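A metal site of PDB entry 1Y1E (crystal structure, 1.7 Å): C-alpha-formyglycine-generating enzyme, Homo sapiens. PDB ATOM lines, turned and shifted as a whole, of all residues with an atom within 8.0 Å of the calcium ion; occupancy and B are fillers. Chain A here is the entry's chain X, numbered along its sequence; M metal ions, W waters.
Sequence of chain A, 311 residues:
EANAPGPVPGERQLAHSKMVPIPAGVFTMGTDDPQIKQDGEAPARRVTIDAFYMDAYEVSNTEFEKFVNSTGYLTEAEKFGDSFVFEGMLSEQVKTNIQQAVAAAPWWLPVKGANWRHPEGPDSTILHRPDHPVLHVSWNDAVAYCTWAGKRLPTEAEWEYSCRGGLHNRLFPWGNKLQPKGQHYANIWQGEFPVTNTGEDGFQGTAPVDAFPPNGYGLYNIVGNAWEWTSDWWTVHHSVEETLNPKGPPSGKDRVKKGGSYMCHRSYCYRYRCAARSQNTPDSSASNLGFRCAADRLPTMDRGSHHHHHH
Within 4 Å of the calcium ion: Glu 58, Asn 221, Gly 224, Ala 226 and Glu 228.
The side-chain carboxylate of Glu 58 sits at hydrogen-bond distance from the side-chain amide nitrogen of Asn 225, at 2.9 Å. NH2 of Arg 292 sits close to O of Asn 221 (3.5 Å). The backbone NH (N) of Gly 224 lies within hydrogen-bond range of the backbone carbonyl oxygen (O) of Gly 260 (3.4 Å). N of Gly 224 sits at hydrogen-bond distance from O of Gly 259, 2.9 Å away. The side-chain carboxylate (OE1) of Glu 228 is in salt-bridge range of the guanidinium group (NE) of Arg 292 (2.8 Å). N of Lys 258 is in hydrogen-bond range of O of Glu 228, 2.8 Å away. The side-chain carboxylate of Glu 228 is in hydrogen-bond range of the indole nitrogen of Trp 159 (2.8 Å).
The calcium ion is bound by OE2 of Glu 58, O of Asn 221, O of Ala 226, water W1, O of Gly 224 and OE2 of Glu 228. The calcium ion has six donor atoms within binding distance.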
ATOM      1  N   TYR A  57      -4.910 -32.342  29.514  1.00  0.00           N
ATOM      2  CA  TYR A  57      -5.097 -30.898  29.322  1.00  0.00           C
ATOM      3  C   TYR A  57      -3.798 -30.131  29.128  1.00  0.00           C
ATOM      4  O   TYR A  57      -2.761 -30.464  29.716  1.00  0.00           O
ATOM      5  CB  TYR A  57      -5.774 -30.301  30.539  1.00  0.00           C
ATOM      6  CG  TYR A  57      -7.009 -31.034  30.995  1.00  0.00           C
ATOM      7  CD1 TYR A  57      -8.182 -31.041  30.213  1.00  0.00           C
ATOM      8  CD2 TYR A  57      -7.024 -31.743  32.198  1.00  0.00           C
ATOM      9  CE1 TYR A  57      -9.311 -31.717  30.618  1.00  0.00           C
ATOM     10  CE2 TYR A  57      -8.165 -32.421  32.619  1.00  0.00           C
ATOM     11  CZ  TYR A  57      -9.314 -32.394  31.833  1.00  0.00           C
ATOM     12  OH  TYR A  57     -10.464 -33.042  32.226  1.00  0.00           O
ATOM     13  N   GLU A  58      -3.898 -29.026  28.393  1.00  0.00           N
ATOM     14  CA  GLU A  58      -2.867 -27.991  28.425  1.00  0.00           C
ATOM     15  C   GLU A  58      -2.666 -27.560  29.875  1.00  0.00           C
ATOM     16  O   GLU A  58      -3.634 -27.522  30.643  1.00  0.00           O
ATOM     17  CB  GLU A  58      -3.297 -26.793  27.611  1.00  0.00           C
ATOM     18  CG  GLU A  58      -3.373 -27.012  26.106  1.00  0.00           C
ATOM     19  CD  GLU A  58      -4.363 -26.093  25.419  1.00  0.00           C
ATOM     20  OE1 GLU A  58      -5.374 -25.725  26.050  1.00  0.00           O
ATOM     21  OE2 GLU A  58      -4.119 -25.725  24.239  1.00  0.00           O
ATOM     22  N   PRO A 133      -5.328 -22.097  29.521  1.00  0.00           N
ATOM     23  CA  PRO A 133      -3.920 -22.448  29.431  1.00  0.00           C
ATOM     24  C   PRO A 133      -2.967 -21.291  29.797  1.00  0.00           C
ATOM     25  O   PRO A 133      -3.224 -20.109  29.493  1.00  0.00           O
ATOM     26  CB  PRO A 133      -3.755 -22.844  27.954  1.00  0.00           C
ATOM     27  CG  PRO A 133      -4.831 -22.130  27.251  1.00  0.00           C
ATOM     28  CD  PRO A 133      -5.989 -22.186  28.204  1.00  0.00           C
ATOM     29  N   TRP A 159       3.786 -36.535  20.607  1.00  0.00           N
ATOM     30  CA  TRP A 159       2.746 -35.517  20.557  1.00  0.00           C
ATOM     31  C   TRP A 159       1.814 -35.792  19.366  1.00  0.00           C
ATOM     32  O   TRP A 159       0.600 -35.878  19.527  1.00  0.00           O
ATOM     33  CB  TRP A 159       3.337 -34.102  20.505  1.00  0.00           C
ATOM     34  CG  TRP A 159       2.300 -33.007  20.654  1.00  0.00           C
ATOM     35  CD1 TRP A 159       2.040 -32.253  21.773  1.00  0.00           C
ATOM     36  CD2 TRP A 159       1.385 -32.555  19.648  1.00  0.00           C
ATOM     37  NE1 TRP A 159       1.011 -31.371  21.513  1.00  0.00           N
ATOM     38  CE2 TRP A 159       0.591 -31.536  20.225  1.00  0.00           C
ATOM     39  CE3 TRP A 159       1.160 -32.902  18.315  1.00  0.00           C
ATOM     40  CZ2 TRP A 159      -0.398 -30.879  19.516  1.00  0.00           C
ATOM     41  CZ3 TRP A 159       0.153 -32.259  17.616  1.00  0.00           C
ATOM     42  CH2 TRP A 159      -0.606 -31.265  18.217  1.00  0.00           C
ATOM     43  N   ASN A 187     -10.747 -24.701  19.384  1.00  0.00           N
ATOM     44  CA  ASN A 187     -10.787 -23.253  19.498  1.00  0.00           C
ATOM     45  C   ASN A 187      -9.778 -22.673  18.532  1.00  0.00           C
ATOM     46  O   ASN A 187      -8.575 -22.630  18.831  1.00  0.00           O
ATOM     47  CB  ASN A 187     -10.522 -22.832  20.932  1.00  0.00           C
ATOM     48  CG  ASN A 187     -10.477 -21.322  21.105  1.00  0.00           C
ATOM     49  OD1 ASN A 187     -11.033 -20.587  20.274  1.00  0.00           O
ATOM     50  ND2 ASN A 187      -9.791 -20.858  22.154  1.00  0.00           N
ATOM     51  N   TYR A 220      -7.737 -33.127  25.376  1.00  0.00           N
ATOM     52  CA  TYR A 220      -8.504 -31.892  25.155  1.00  0.00           C
ATOM     53  C   TYR A 220      -7.606 -30.841  24.507  1.00  0.00           C
ATOM     54  O   TYR A 220      -6.484 -30.661  24.940  1.00  0.00           O
ATOM     55  CB  TYR A 220      -9.019 -31.364  26.506  1.00  0.00           C
ATOM     56  CG  TYR A 220     -10.098 -32.249  27.082  1.00  0.00           C
ATOM     57  CD1 TYR A 220      -9.773 -33.429  27.747  1.00  0.00           C
ATOM     58  CD2 TYR A 220     -11.448 -31.933  26.898  1.00  0.00           C
ATOM     59  CE1 TYR A 220     -10.764 -34.268  28.231  1.00  0.00           C
ATOM     60  CE2 TYR A 220     -12.442 -32.752  27.382  1.00  0.00           C
ATOM     61  CZ  TYR A 220     -12.088 -33.918  28.058  1.00  0.00           C
ATOM     62  OH  TYR A 220     -13.074 -34.726  28.562  1.00  0.00           O
ATOM     63  N   ASN A 221      -8.124 -30.177  23.470  1.00  0.00           N
ATOM     64  CA  ASN A 221      -7.496 -29.005  22.840  1.00  0.00           C
ATOM     65  C   ASN A 221      -6.073 -29.235  22.391  1.00  0.00           C
ATOM     66  O   ASN A 221      -5.224 -28.349  22.457  1.00  0.00           O
ATOM     67  CB  ASN A 221      -7.578 -27.774  23.754  1.00  0.00           C
ATOM     68  CG  ASN A 221      -8.990 -27.450  24.124  1.00  0.00           C
ATOM     69  OD1 ASN A 221      -9.776 -26.963  23.291  1.00  0.00           O
ATOM     70  ND2 ASN A 221      -9.353 -27.777  25.372  1.00  0.00           N
ATOM     71  N   ILE A 222      -5.839 -30.453  21.926  1.00  0.00           N
ATOM     72  CA  ILE A 222      -4.554 -30.823  21.383  1.00  0.00           C
ATOM     73  C   ILE A 222      -4.306 -30.127  20.038  1.00  0.00           C
ATOM     74  O   ILE A 222      -3.168 -29.826  19.738  1.00  0.00           O
ATOM     75  CB  ILE A 222      -4.411 -32.387  21.303  1.00  0.00           C
ATOM     76  CG1 ILE A 222      -2.962 -32.748  20.992  1.00  0.00           C
ATOM     77  CG2 ILE A 222      -5.385 -32.987  20.311  1.00  0.00           C
ATOM     78  CD1 ILE A 222      -2.288 -33.520  22.042  1.00  0.00           C
ATOM     79  N   VAL A 223      -5.355 -29.852  19.258  1.00  0.00           N
ATOM     80  CA  VAL A 223      -5.257 -28.812  18.236  1.00  0.00           C
ATOM     81  C   VAL A 223      -6.047 -27.597  18.706  1.00  0.00           C
ATOM     82  O   VAL A 223      -7.067 -27.716  19.402  1.00  0.00           O
ATOM     83  CB  VAL A 223      -5.666 -29.254  16.781  1.00  0.00           C
ATOM     84  CG1 VAL A 223      -4.844 -30.415  16.343  1.00  0.00           C
ATOM     85  CG2 VAL A 223      -7.161 -29.568  16.669  1.00  0.00           C
ATOM     86  N   GLY A 224      -5.526 -26.437  18.357  1.00  0.00           N
ATOM     87  CA  GLY A 224      -6.117 -25.150  18.733  1.00  0.00           C
ATOM     88  C   GLY A 224      -5.888 -24.755  20.186  1.00  0.00           C
ATOM     89  O   GLY A 224      -5.191 -25.425  20.917  1.00  0.00           O
ATOM     90  N   ASN A 225      -6.497 -23.631  20.564  1.00  0.00           N
ATOM     91  CA  ASN A 225      -6.382 -23.038  21.899  1.00  0.00           C
ATOM     92  C   ASN A 225      -4.948 -22.512  22.070  1.00  0.00           C
ATOM     93  O   ASN A 225      -4.637 -21.480  21.488  1.00  0.00           O
ATOM     94  CB  ASN A 225      -6.874 -23.988  22.994  1.00  0.00           C
ATOM     95  CG  ASN A 225      -7.553 -23.258  24.140  1.00  0.00           C
ATOM     96  OD1 ASN A 225      -8.199 -22.227  23.930  1.00  0.00           O
ATOM     97  ND2 ASN A 225      -7.427 -23.793  25.344  1.00  0.00           N
ATOM     98  N   ALA A 226      -4.074 -23.196  22.804  1.00  0.00           N
ATOM     99  CA  ALA A 226      -2.663 -22.771  22.807  1.00  0.00           C
ATOM    100  C   ALA A 226      -1.812 -23.684  21.950  1.00  0.00           C
ATOM    101  O   ALA A 226      -2.004 -24.897  21.970  1.00  0.00           O
ATOM    102  CB  ALA A 226      -2.114 -22.742  24.234  1.00  0.00           C
ATOM    103  N   TRP A 227      -0.842 -23.126  21.226  1.00  0.00           N
ATOM    104  CA  TRP A 227       0.262 -23.929  20.716  1.00  0.00           C
ATOM    105  C   TRP A 227       0.936 -24.723  21.837  1.00  0.00           C
ATOM    106  O   TRP A 227       0.872 -24.355  22.998  1.00  0.00           O
ATOM    107  CB  TRP A 227       1.352 -23.052  20.110  1.00  0.00           C
ATOM    108  CG  TRP A 227       1.159 -22.583  18.724  1.00  0.00           C
ATOM    109  CD1 TRP A 227       0.735 -21.343  18.331  1.00  0.00           C
ATOM    110  CD2 TRP A 227       1.481 -23.296  17.531  1.00  0.00           C
ATOM    111  NE1 TRP A 227       0.737 -21.260  16.936  1.00  0.00           N
ATOM    112  CE2 TRP A 227       1.186 -22.455  16.432  1.00  0.00           C
ATOM    113  CE3 TRP A 227       1.968 -24.582  17.279  1.00  0.00           C
ATOM    114  CZ2 TRP A 227       1.381 -22.849  15.101  1.00  0.00           C
ATOM    115  CZ3 TRP A 227       2.156 -24.978  15.956  1.00  0.00           C
ATOM    116  CH2 TRP A 227       1.857 -24.118  14.893  1.00  0.00           C
ATOM    117  N   GLU A 228       1.599 -25.818  21.465  1.00  0.00           N
ATOM    118  CA  GLU A 228       2.217 -26.699  22.459  1.00  0.00           C
ATOM    119  C   GLU A 228       3.663 -27.030  22.163  1.00  0.00           C
ATOM    120  O   GLU A 228       3.988 -27.552  21.085  1.00  0.00           O
ATOM    121  CB  GLU A 228       1.364 -27.954  22.614  1.00  0.00           C
ATOM    122  CG  GLU A 228      -0.075 -27.562  22.923  1.00  0.00           C
ATOM    123  CD  GLU A 228      -1.002 -28.730  23.211  1.00  0.00           C
ATOM    124  OE1 GLU A 228      -0.535 -29.876  23.312  1.00  0.00           O
ATOM    125  OE2 GLU A 228      -2.215 -28.462  23.358  1.00  0.00           O
ATOM    126  N   LYS A 258       3.639 -27.590  18.284  1.00  0.00           N
ATOM    127  CA  LYS A 258       2.604 -28.275  17.523  1.00  0.00           C
ATOM    128  C   LYS A 258       1.214 -27.806  17.904  1.00  0.00           C
ATOM    129  O   LYS A 258       0.992 -27.238  18.988  1.00  0.00           O
ATOM    130  CB  LYS A 258       2.685 -29.805  17.739  1.00  0.00           C
ATOM    131  CG  LYS A 258       4.012 -30.436  17.354  1.00  0.00           C
ATOM    132  CD  LYS A 258       4.106 -30.720  15.852  1.00  0.00           C
ATOM    133  CE  LYS A 258       3.462 -32.074  15.511  1.00  0.00           C
ATOM    134  NZ  LYS A 258       3.623 -32.440  14.036  1.00  0.00           N
ATOM    135  N   GLY A 259       0.281 -28.047  16.978  1.00  0.00           N
ATOM    136  CA  GLY A 259      -1.131 -28.034  17.268  1.00  0.00           C
ATOM    137  C   GLY A 259      -1.939 -26.801  16.868  1.00  0.00           C
ATOM    138  O   GLY A 259      -3.155 -26.882  16.779  1.00  0.00           O
ATOM    139  N   GLY A 260      -1.277 -25.675  16.656  1.00  0.00           N
ATOM    140  CA  GLY A 260      -2.000 -24.462  16.364  1.00  0.00           C
ATOM    141  C   GLY A 260      -2.725 -23.892  17.568  1.00  0.00           C
ATOM    142  O   GLY A 260      -2.718 -24.492  18.638  1.00  0.00           O
ATOM    143  N   SER A 261      -3.280 -22.686  17.373  1.00  0.00           N
ATOM    144  CA  SER A 261      -3.861 -21.888  18.426  1.00  0.00           C
ATOM    145  C   SER A 261      -5.226 -21.276  18.059  1.00  0.00           C
ATOM    146  O   SER A 261      -5.720 -21.406  16.946  1.00  0.00           O
ATOM    147  CB  SER A 261      -2.907 -20.751  18.777  1.00  0.00           C
ATOM    148  OG  SER A 261      -2.971 -19.687  17.851  1.00  0.00           O
ATOM    149  N   TYR A 262      -5.784 -20.564  19.030  1.00  0.00           N
ATOM    150  CA  TYR A 262      -7.006 -19.752  18.806  1.00  0.00           C
ATOM    151  C   TYR A 262      -6.916 -18.701  17.692  1.00  0.00           C
ATOM    152  O   TYR A 262      -7.939 -18.138  17.281  1.00  0.00           O
ATOM    153  CB  TYR A 262      -7.441 -19.090  20.108  1.00  0.00           C
ATOM    154  CG  TYR A 262      -6.571 -17.968  20.608  1.00  0.00           C
ATOM    155  CD1 TYR A 262      -5.641 -18.166  21.634  1.00  0.00           C
ATOM    156  CD2 TYR A 262      -6.709 -16.682  20.094  1.00  0.00           C
ATOM    157  CE1 TYR A 262      -4.845 -17.115  22.095  1.00  0.00           C
ATOM    158  CE2 TYR A 262      -5.940 -15.636  20.558  1.00  0.00           C
ATOM    159  CZ  TYR A 262      -5.018 -15.854  21.564  1.00  0.00           C
ATOM    160  OH  TYR A 262      -4.256 -14.819  22.023  1.00  0.00           O
ATOM    161  N   ASN A 288      -0.051 -16.927  22.521  1.00  0.00           N
ATOM    162  CA  ASN A 288      -0.804 -18.081  22.003  1.00  0.00           C
ATOM    163  C   ASN A 288      -0.065 -19.389  22.156  1.00  0.00           C
ATOM    164  O   ASN A 288      -0.396 -20.353  21.461  1.00  0.00           O
ATOM    165  CB  ASN A 288      -1.150 -17.886  20.518  1.00  0.00           C
ATOM    166  CG  ASN A 288       0.068 -17.883  19.628  1.00  0.00           C
ATOM    167  OD1 ASN A 288       1.183 -17.746  20.111  1.00  0.00           O
ATOM    168  ND2 ASN A 288      -0.137 -18.065  18.307  1.00  0.00           N
ATOM    169  N   GLY A 290       1.746 -22.331  24.692  1.00  0.00           N
ATOM    170  CA  GLY A 290       1.808 -22.979  25.984  1.00  0.00           C
ATOM    171  C   GLY A 290       2.316 -24.406  25.828  1.00  0.00           C
ATOM    172  O   GLY A 290       3.180 -24.690  24.976  1.00  0.00           O
ATOM    173  N   PHE A 291       1.773 -25.306  26.631  1.00  0.00           N
ATOM    174  CA  PHE A 291       2.292 -26.694  26.638  1.00  0.00           C
ATOM    175  C   PHE A 291       1.472 -27.637  27.482  1.00  0.00           C
ATOM    176  O   PHE A 291       0.647 -27.205  28.307  1.00  0.00           O
ATOM    177  CB  PHE A 291       3.770 -26.736  27.138  1.00  0.00           C
ATOM    178  CG  PHE A 291       3.934 -26.422  28.608  1.00  0.00           C
ATOM    179  CD1 PHE A 291       4.213 -27.433  29.524  1.00  0.00           C
ATOM    180  CD2 PHE A 291       3.825 -25.124  29.076  1.00  0.00           C
ATOM    181  CE1 PHE A 291       4.379 -27.136  30.893  1.00  0.00           C
ATOM    182  CE2 PHE A 291       3.964 -24.832  30.450  1.00  0.00           C
ATOM    183  CZ  PHE A 291       4.236 -25.823  31.338  1.00  0.00           C
ATOM    184  N   ARG A 292       1.761 -28.935  27.295  1.00  0.00           N
ATOM    185  CA  ARG A 292       1.320 -30.003  28.175  1.00  0.00           C
ATOM    186  C   ARG A 292       2.507 -30.942  28.418  1.00  0.00           C
ATOM    187  O   ARG A 292       3.470 -30.961  27.637  1.00  0.00           O
ATOM    188  CB  ARG A 292       0.120 -30.758  27.596  1.00  0.00           C
ATOM    189  CG  ARG A 292       0.427 -31.768  26.477  1.00  0.00           C
ATOM    190  CD  ARG A 292      -0.845 -32.454  25.966  1.00  0.00           C
ATOM    191  NE  ARG A 292      -1.709 -31.516  25.274  1.00  0.00           N
ATOM    192  CZ  ARG A 292      -3.039 -31.466  25.381  1.00  0.00           C
ATOM    193  NH1 ARG A 292      -3.693 -32.312  26.172  1.00  0.00           N
ATOM    194  NH2 ARG A 292      -3.711 -30.550  24.688  1.00  0.00           N
HETATM  195 CA    CA M   1      -3.560 -26.677  22.252  1.00  0.00          CA
HETATM  196  O   HOH W   1      -2.512 -26.943  20.093  1.00  0.00           O
